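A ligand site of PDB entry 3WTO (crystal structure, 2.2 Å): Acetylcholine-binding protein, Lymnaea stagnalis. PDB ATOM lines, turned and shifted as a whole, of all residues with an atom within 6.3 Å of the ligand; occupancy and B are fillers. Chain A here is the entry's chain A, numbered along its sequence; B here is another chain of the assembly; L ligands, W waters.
The backbone carbonyl oxygen (O) of Trp 147 sits at hydrogen-bond distance from a nitrogen (N1) of the ligand, 2.8 Å away.
The backbone carbonyl oxygen of Ser 146 sits at hydrogen-bond distance from a nitrogen (N1) of the ligand, 3.4 Å away.
A nitrogen (N1) of the ligand lies within hydrogen-bond range of the side-chain hydroxyl (OH) of Tyr 93, at 3.0 Å.
The indole nitrogen (NE1) of Trp 147 sits at hydrogen-bond distance from the side-chain hydroxyl (OG1) of Thr 103 of chain B.
The side-chain hydroxyl (OH) of Tyr 168 of chain B sits at hydrogen-bond distance from the backbone NH (N) of Cys 191 (2.8 Å).
The backbone NH (N) of Arg 108 of chain B sits at hydrogen-bond distance from the backbone carbonyl oxygen (O) of Leu 116 of chain B (2.8 Å).
N of His 149 lies within hydrogen-bond range of OG of Ser 146, at 2.8 Å.
The guanidinium group (NH1) of Arg 108 of chain B lies within hydrogen-bond range of a ring nitrogen (ND1) of His 149, at 3.5 Å.
The backbone carbonyl oxygen (O) of Met 118 of chain B lies close to the indole nitrogen (NE1) of Trp 147 (3.3 Å).
The backbone NH (N) of Tyr 196 lies within hydrogen-bond range of the backbone carbonyl oxygen (O) of Val 187.
The side-chain sulfur (SG) of Cys 191 forms a disulfide with the side-chain sulfur (SG) of Cys 192.
Merely in contact with the ligand: Arg 108 of chain B, Leu 116 of chain B, Tyr 196, Met 118 of chain B, Tyr 189, Cys 191, Thr 148, Cys 192 and Trp 57 of chain B.
Hydrophobic or aromatic side chains within 4 Å of the ligand: Tyr 93, Trp 147, Tyr 189, Tyr 196, Trp 57 of chain B, Leu 116 of chain B and Met 118 of chain B.
12 residues have an atom within 4 Å of the ligand: Tyr 93, Ser 146, Trp 147, Thr 148, Tyr 189, Cys 191, Cys 192, Tyr 196, Trp 57 of chain B, Arg 108 of chain B, Leu 116 of chain B and Met 118 of chain B.
The nearest printed residue that does not touch the ligand is Ala 107 of chain B (4.02 Å).
Water W1 lies within hydrogen-bond range of a nitrogen (N4) of the ligand (2.7 Å), the backbone carbonyl oxygen (O) of Leu 106 of chain B (2.8 Å), the backbone NH (N) of Met 118 of chain B (3.1 Å) and the indole nitrogen (NE1) of Trp 147 (3.4 Å).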
ATOM      1  N   TYR A  93      14.953 -14.024  23.192  1.00  0.00           N
ATOM      2  CA  TYR A  93      16.256 -14.661  23.040  1.00  0.00           C
ATOM      3  C   TYR A  93      16.796 -15.325  24.305  1.00  0.00           C
ATOM      4  O   TYR A  93      17.369 -16.425  24.243  1.00  0.00           O
ATOM      5  CB  TYR A  93      17.301 -13.660  22.538  1.00  0.00           C
ATOM      6  CG  TYR A  93      17.188 -13.307  21.072  1.00  0.00           C
ATOM      7  CD1 TYR A  93      18.100 -13.807  20.144  1.00  0.00           C
ATOM      8  CD2 TYR A  93      16.190 -12.448  20.623  1.00  0.00           C
ATOM      9  CE1 TYR A  93      18.019 -13.463  18.791  1.00  0.00           C
ATOM     10  CE2 TYR A  93      16.097 -12.100  19.267  1.00  0.00           C
ATOM     11  CZ  TYR A  93      17.014 -12.615  18.362  1.00  0.00           C
ATOM     12  OH  TYR A  93      16.934 -12.256  17.018  1.00  0.00           O
ATOM     13  N   GLY A 145      12.403 -10.347  19.658  1.00  0.00           N
ATOM     14  CA  GLY A 145      12.423  -9.972  18.245  1.00  0.00           C
ATOM     15  C   GLY A 145      11.926 -11.092  17.343  1.00  0.00           C
ATOM     16  O   GLY A 145      11.650 -12.199  17.814  1.00  0.00           O
ATOM     17  N   SER A 146      11.818 -10.828  16.048  1.00  0.00           N
ATOM     18  CA  SER A 146      11.348 -11.871  15.137  1.00  0.00           C
ATOM     19  C   SER A 146      12.392 -12.965  15.040  1.00  0.00           C
ATOM     20  O   SER A 146      13.585 -12.693  14.847  1.00  0.00           O
ATOM     21  CB  SER A 146      11.074 -11.308  13.739  1.00  0.00           C
ATOM     22  OG  SER A 146      10.844 -12.354  12.826  1.00  0.00           O
ATOM     23  N   TRP A 147      11.960 -14.209  15.166  1.00  0.00           N
ATOM     24  CA  TRP A 147      12.875 -15.322  15.109  1.00  0.00           C
ATOM     25  C   TRP A 147      13.381 -15.583  13.687  1.00  0.00           C
ATOM     26  O   TRP A 147      14.566 -15.803  13.485  1.00  0.00           O
ATOM     27  CB  TRP A 147      12.214 -16.573  15.706  1.00  0.00           C
ATOM     28  CG  TRP A 147      13.126 -17.749  15.847  1.00  0.00           C
ATOM     29  CD1 TRP A 147      12.994 -18.955  15.229  1.00  0.00           C
ATOM     30  CD2 TRP A 147      14.314 -17.834  16.640  1.00  0.00           C
ATOM     31  NE1 TRP A 147      14.021 -19.792  15.592  1.00  0.00           N
ATOM     32  CE2 TRP A 147      14.849 -19.130  16.458  1.00  0.00           C
ATOM     33  CE3 TRP A 147      14.989 -16.933  17.489  1.00  0.00           C
ATOM     34  CZ2 TRP A 147      16.024 -19.551  17.093  1.00  0.00           C
ATOM     35  CZ3 TRP A 147      16.156 -17.364  18.119  1.00  0.00           C
ATOM     36  CH2 TRP A 147      16.666 -18.660  17.918  1.00  0.00           C
ATOM     37  N   THR A 148      12.492 -15.524  12.699  1.00  0.00           N
ATOM     38  CA  THR A 148      12.899 -15.801  11.323  1.00  0.00           C
ATOM     39  C   THR A 148      12.777 -14.682  10.288  1.00  0.00           C
ATOM     40  O   THR A 148      13.231 -14.840   9.149  1.00  0.00           O
ATOM     41  CB  THR A 148      12.115 -17.003  10.750  1.00  0.00           C
ATOM     42  OG1 THR A 148      10.740 -16.639  10.576  1.00  0.00           O
ATOM     43  CG2 THR A 148      12.216 -18.200  11.692  1.00  0.00           C
ATOM     44  N   HIS A 149      12.162 -13.559  10.641  1.00  0.00           N
ATOM     45  CA  HIS A 149      12.041 -12.480   9.674  1.00  0.00           C
ATOM     46  C   HIS A 149      13.102 -11.390   9.937  1.00  0.00           C
ATOM     47  O   HIS A 149      13.100 -10.764  10.987  1.00  0.00           O
ATOM     48  CB  HIS A 149      10.622 -11.894   9.718  1.00  0.00           C
ATOM     49  CG  HIS A 149       9.580 -12.804   9.141  1.00  0.00           C
ATOM     50  ND1 HIS A 149       9.531 -13.126   7.798  1.00  0.00           N
ATOM     51  CD2 HIS A 149       8.557 -13.471   9.722  1.00  0.00           C
ATOM     52  CE1 HIS A 149       8.517 -13.954   7.575  1.00  0.00           C
ATOM     53  NE2 HIS A 149       7.905 -14.177   8.734  1.00  0.00           N
ATOM     54  N   VAL A 187      20.902  -6.349  14.848  1.00  0.00           N
ATOM     55  CA  VAL A 187      22.118  -7.141  14.906  1.00  0.00           C
ATOM     56  C   VAL A 187      22.332  -8.153  13.788  1.00  0.00           C
ATOM     57  O   VAL A 187      21.410  -8.855  13.370  1.00  0.00           O
ATOM     58  CB  VAL A 187      22.188  -7.917  16.252  1.00  0.00           C
ATOM     59  CG1 VAL A 187      23.587  -8.455  16.467  1.00  0.00           C
ATOM     60  CG2 VAL A 187      21.750  -7.017  17.407  1.00  0.00           C
ATOM     61  N   TYR A 189      24.231 -11.512  13.041  1.00  0.00           N
ATOM     62  CA  TYR A 189      24.907 -12.611  13.739  1.00  0.00           C
ATOM     63  C   TYR A 189      25.778 -13.386  12.745  1.00  0.00           C
ATOM     64  O   TYR A 189      25.471 -13.424  11.544  1.00  0.00           O
ATOM     65  CB  TYR A 189      23.880 -13.560  14.377  1.00  0.00           C
ATOM     66  CG  TYR A 189      22.874 -12.881  15.273  1.00  0.00           C
ATOM     67  CD1 TYR A 189      21.942 -11.980  14.761  1.00  0.00           C
ATOM     68  CD2 TYR A 189      22.860 -13.117  16.644  1.00  0.00           C
ATOM     69  CE1 TYR A 189      21.016 -11.352  15.576  1.00  0.00           C
ATOM     70  CE2 TYR A 189      21.934 -12.490  17.484  1.00  0.00           C
ATOM     71  CZ  TYR A 189      21.014 -11.606  16.942  1.00  0.00           C
ATOM     72  OH  TYR A 189      20.113 -10.962  17.762  1.00  0.00           O
ATOM     73  N   CYS A 191      26.034 -16.430  12.270  1.00  0.00           N
ATOM     74  CA  CYS A 191      25.254 -17.525  11.686  1.00  0.00           C
ATOM     75  C   CYS A 191      24.563 -17.155  10.408  1.00  0.00           C
ATOM     76  O   CYS A 191      24.429 -17.972   9.497  1.00  0.00           O
ATOM     77  CB  CYS A 191      24.113 -17.941  12.602  1.00  0.00           C
ATOM     78  SG  CYS A 191      22.668 -16.772  12.686  1.00  0.00           S
ATOM     79  N   CYS A 192      24.110 -15.924  10.365  1.00  0.00           N
ATOM     80  CA  CYS A 192      23.275 -15.518   9.273  1.00  0.00           C
ATOM     81  C   CYS A 192      23.622 -14.193   8.567  1.00  0.00           C
ATOM     82  O   CYS A 192      24.104 -13.245   9.183  1.00  0.00           O
ATOM     83  CB  CYS A 192      21.876 -15.515   9.868  1.00  0.00           C
ATOM     84  SG  CYS A 192      21.520 -16.945  10.990  1.00  0.00           S
ATOM     85  N   TYR A 196      18.778  -8.906  12.107  1.00  0.00           N
ATOM     86  CA  TYR A 196      17.519  -9.108  12.842  1.00  0.00           C
ATOM     87  C   TYR A 196      17.351  -8.053  13.909  1.00  0.00           C
ATOM     88  O   TYR A 196      18.275  -7.757  14.659  1.00  0.00           O
ATOM     89  CB  TYR A 196      17.485 -10.484  13.519  1.00  0.00           C
ATOM     90  CG  TYR A 196      17.550 -11.632  12.551  1.00  0.00           C
ATOM     91  CD1 TYR A 196      18.785 -12.122  12.099  1.00  0.00           C
ATOM     92  CD2 TYR A 196      16.388 -12.174  12.019  1.00  0.00           C
ATOM     93  CE1 TYR A 196      18.841 -13.124  11.146  1.00  0.00           C
ATOM     94  CE2 TYR A 196      16.438 -13.178  11.058  1.00  0.00           C
ATOM     95  CZ  TYR A 196      17.666 -13.649  10.619  1.00  0.00           C
ATOM     96  OH  TYR A 196      17.699 -14.605   9.648  1.00  0.00           O
ATOM     97  N   TRP B  57      20.743 -23.799  19.797  1.00  0.00           N
ATOM     98  CA  TRP B  57      20.104 -23.591  18.503  1.00  0.00           C
ATOM     99  C   TRP B  57      20.537 -24.810  17.693  1.00  0.00           C
ATOM    100  O   TRP B  57      21.721 -25.136  17.670  1.00  0.00           O
ATOM    101  CB  TRP B  57      20.667 -22.355  17.816  1.00  0.00           C
ATOM    102  CG  TRP B  57      20.305 -21.072  18.457  1.00  0.00           C
ATOM    103  CD1 TRP B  57      19.437 -20.884  19.489  1.00  0.00           C
ATOM    104  CD2 TRP B  57      20.774 -19.787  18.079  1.00  0.00           C
ATOM    105  NE1 TRP B  57      19.333 -19.544  19.776  1.00  0.00           N
ATOM    106  CE2 TRP B  57      20.147 -18.850  18.927  1.00  0.00           C
ATOM    107  CE3 TRP B  57      21.678 -19.325  17.105  1.00  0.00           C
ATOM    108  CZ2 TRP B  57      20.377 -17.469  18.825  1.00  0.00           C
ATOM    109  CZ3 TRP B  57      21.912 -17.958  17.002  1.00  0.00           C
ATOM    110  CH2 TRP B  57      21.256 -17.039  17.862  1.00  0.00           C
ATOM    111  N   THR B 103      11.167 -21.706  20.306  1.00  0.00           N
ATOM    112  CA  THR B 103      10.895 -20.701  19.283  1.00  0.00           C
ATOM    113  C   THR B 103       9.811 -21.072  18.277  1.00  0.00           C
ATOM    114  O   THR B 103       9.411 -22.227  18.182  1.00  0.00           O
ATOM    115  CB  THR B 103      12.197 -20.379  18.545  1.00  0.00           C
ATOM    116  OG1 THR B 103      12.743 -21.578  18.009  1.00  0.00           O
ATOM    117  CG2 THR B 103      13.201 -19.748  19.507  1.00  0.00           C
ATOM    118  N   LEU B 106       9.129 -22.250  12.478  1.00  0.00           N
ATOM    119  CA  LEU B 106       9.146 -21.802  11.100  1.00  0.00           C
ATOM    120  C   LEU B 106      10.531 -22.037  10.536  1.00  0.00           C
ATOM    121  O   LEU B 106      11.526 -21.924  11.238  1.00  0.00           O
ATOM    122  CB  LEU B 106       8.830 -20.303  11.048  1.00  0.00           C
ATOM    123  CG  LEU B 106       7.515 -19.849  11.646  1.00  0.00           C
ATOM    124  CD1 LEU B 106       7.470 -18.340  11.678  1.00  0.00           C
ATOM    125  CD2 LEU B 106       6.363 -20.397  10.840  1.00  0.00           C
ATOM    126  N   ALA B 107      10.573 -22.397   9.261  1.00  0.00           N
ATOM    127  CA  ALA B 107      11.843 -22.599   8.573  1.00  0.00           C
ATOM    128  C   ALA B 107      11.877 -21.571   7.451  1.00  0.00           C
ATOM    129  O   ALA B 107      10.835 -21.017   7.078  1.00  0.00           O
ATOM    130  CB  ALA B 107      11.918 -24.027   8.005  1.00  0.00           C
ATOM    131  N   ARG B 108      13.066 -21.299   6.932  1.00  0.00           N
ATOM    132  CA  ARG B 108      13.208 -20.382   5.820  1.00  0.00           C
ATOM    133  C   ARG B 108      13.451 -21.251   4.581  1.00  0.00           C
ATOM    134  O   ARG B 108      14.271 -22.169   4.611  1.00  0.00           O
ATOM    135  CB  ARG B 108      14.408 -19.442   6.030  1.00  0.00           C
ATOM    136  CG  ARG B 108      14.220 -18.366   7.106  1.00  0.00           C
ATOM    137  CD  ARG B 108      13.165 -17.312   6.720  1.00  0.00           C
ATOM    138  NE  ARG B 108      13.656 -16.330   5.752  1.00  0.00           N
ATOM    139  CZ  ARG B 108      12.985 -15.237   5.393  1.00  0.00           C
ATOM    140  NH1 ARG B 108      11.794 -14.991   5.924  1.00  0.00           N
ATOM    141  NH2 ARG B 108      13.522 -14.386   4.529  1.00  0.00           N
ATOM    142  N   LEU B 116      16.295 -23.974   5.651  1.00  0.00           N
ATOM    143  CA  LEU B 116      16.997 -23.758   6.894  1.00  0.00           C
ATOM    144  C   LEU B 116      15.972 -23.820   8.019  1.00  0.00           C
ATOM    145  O   LEU B 116      14.909 -23.198   7.952  1.00  0.00           O
ATOM    146  CB  LEU B 116      17.703 -22.393   6.927  1.00  0.00           C
ATOM    147  CG  LEU B 116      18.167 -21.910   8.315  1.00  0.00           C
ATOM    148  CD1 LEU B 116      19.249 -22.820   8.900  1.00  0.00           C
ATOM    149  CD2 LEU B 116      18.676 -20.488   8.213  1.00  0.00           C
ATOM    150  N   TYR B 117      16.294 -24.588   9.048  1.00  0.00           N
ATOM    151  CA  TYR B 117      15.426 -24.715  10.201  1.00  0.00           C
ATOM    152  C   TYR B 117      16.349 -24.719  11.400  1.00  0.00           C
ATOM    153  O   TYR B 117      17.177 -25.611  11.578  1.00  0.00           O
ATOM    154  CB  TYR B 117      14.595 -26.003  10.140  1.00  0.00           C
ATOM    155  CG  TYR B 117      13.666 -26.146  11.337  1.00  0.00           C
ATOM    156  CD1 TYR B 117      12.930 -25.049  11.801  1.00  0.00           C
ATOM    157  CD2 TYR B 117      13.586 -27.345  12.047  1.00  0.00           C
ATOM    158  CE1 TYR B 117      12.145 -25.146  12.954  1.00  0.00           C
ATOM    159  CE2 TYR B 117      12.808 -27.446  13.197  1.00  0.00           C
ATOM    160  CZ  TYR B 117      12.091 -26.349  13.648  1.00  0.00           C
ATOM    161  OH  TYR B 117      11.347 -26.424  14.806  1.00  0.00           O
ATOM    162  N   MET B 118      16.218 -23.693  12.240  1.00  0.00           N
ATOM    163  CA  MET B 118      17.089 -23.586  13.392  1.00  0.00           C
ATOM    164  C   MET B 118      16.323 -23.245  14.655  1.00  0.00           C
ATOM    165  O   MET B 118      16.269 -22.097  15.092  1.00  0.00           O
ATOM    166  CB  MET B 118      18.172 -22.544  13.100  1.00  0.00           C
ATOM    167  CG  MET B 118      19.224 -22.428  14.177  1.00  0.00           C
ATOM    168  SD  MET B 118      20.589 -21.363  13.656  1.00  0.00           S
ATOM    169  CE  MET B 118      19.826 -19.787  13.803  1.00  0.00           C
ATOM    170  N   PRO B 119      15.710 -24.254  15.271  1.00  0.00           N
ATOM    171  CA  PRO B 119      14.956 -24.013  16.497  1.00  0.00           C
ATOM    172  C   PRO B 119      15.872 -23.930  17.708  1.00  0.00           C
ATOM    173  O   PRO B 119      16.914 -24.595  17.736  1.00  0.00           O
ATOM    174  CB  PRO B 119      14.030 -25.213  16.567  1.00  0.00           C
ATOM    175  CG  PRO B 119      14.888 -26.307  15.997  1.00  0.00           C
ATOM    176  CD  PRO B 119      15.463 -25.620  14.773  1.00  0.00           C
ATOM    177  N   TYR B 168      27.164 -16.943  21.225  1.00  0.00           N
ATOM    178  CA  TYR B 168      25.762 -16.702  21.544  1.00  0.00           C
ATOM    179  C   TYR B 168      25.457 -17.188  22.951  1.00  0.00           C
ATOM    180  O   TYR B 168      24.364 -16.959  23.467  1.00  0.00           O
ATOM    181  CB  TYR B 168      24.863 -17.437  20.557  1.00  0.00           C
ATOM    182  CG  TYR B 168      25.220 -17.231  19.096  1.00  0.00           C
ATOM    183  CD1 TYR B 168      25.300 -15.950  18.553  1.00  0.00           C
ATOM    184  CD2 TYR B 168      25.458 -18.316  18.257  1.00  0.00           C
ATOM    185  CE1 TYR B 168      25.593 -15.757  17.199  1.00  0.00           C
ATOM    186  CE2 TYR B 168      25.753 -18.145  16.906  1.00  0.00           C
ATOM    187  CZ  TYR B 168      25.828 -16.853  16.388  1.00  0.00           C
ATOM    188  OH  TYR B 168      26.134 -16.679  15.053  1.00  0.00           O
HETATM  189  N1  LIG L   1      16.493 -14.462  15.021  1.00  0.00           N
HETATM  190  N2  LIG L   1      18.019 -16.222  14.546  1.00  0.00           N
HETATM  191  C1  LIG L   1      17.689 -14.864  14.798  1.00  0.00           C
HETATM  192  N3  LIG L   1      18.833 -14.053  14.765  1.00  0.00           N
HETATM  193  C2  LIG L   1      20.007 -14.873  14.479  1.00  0.00           C
HETATM  194  C3  LIG L   1      19.471 -16.314  14.323  1.00  0.00           C
HETATM  195  C4  LIG L   1      15.681 -19.408  10.923  1.00  0.00           C
HETATM  196 CL1  LIG L   1      15.049 -20.346   9.589  1.00  0.00          CL
HETATM  197  N4  LIG L   1      15.602 -19.953  12.129  1.00  0.00           N
HETATM  198  C5  LIG L   1      16.047 -19.327  13.221  1.00  0.00           C
HETATM  199  C6  LIG L   1      16.640 -18.036  13.173  1.00  0.00           C
HETATM  200  C7  LIG L   1      16.745 -17.424  11.876  1.00  0.00           C
HETATM  201  C8  LIG L   1      16.267 -18.112  10.720  1.00  0.00           C
HETATM  202  C9  LIG L   1      17.112 -17.403  14.490  1.00  0.00           C
HETATM  203  O   HOH W   1      13.840 -21.833  12.877  1.00  0.00           O
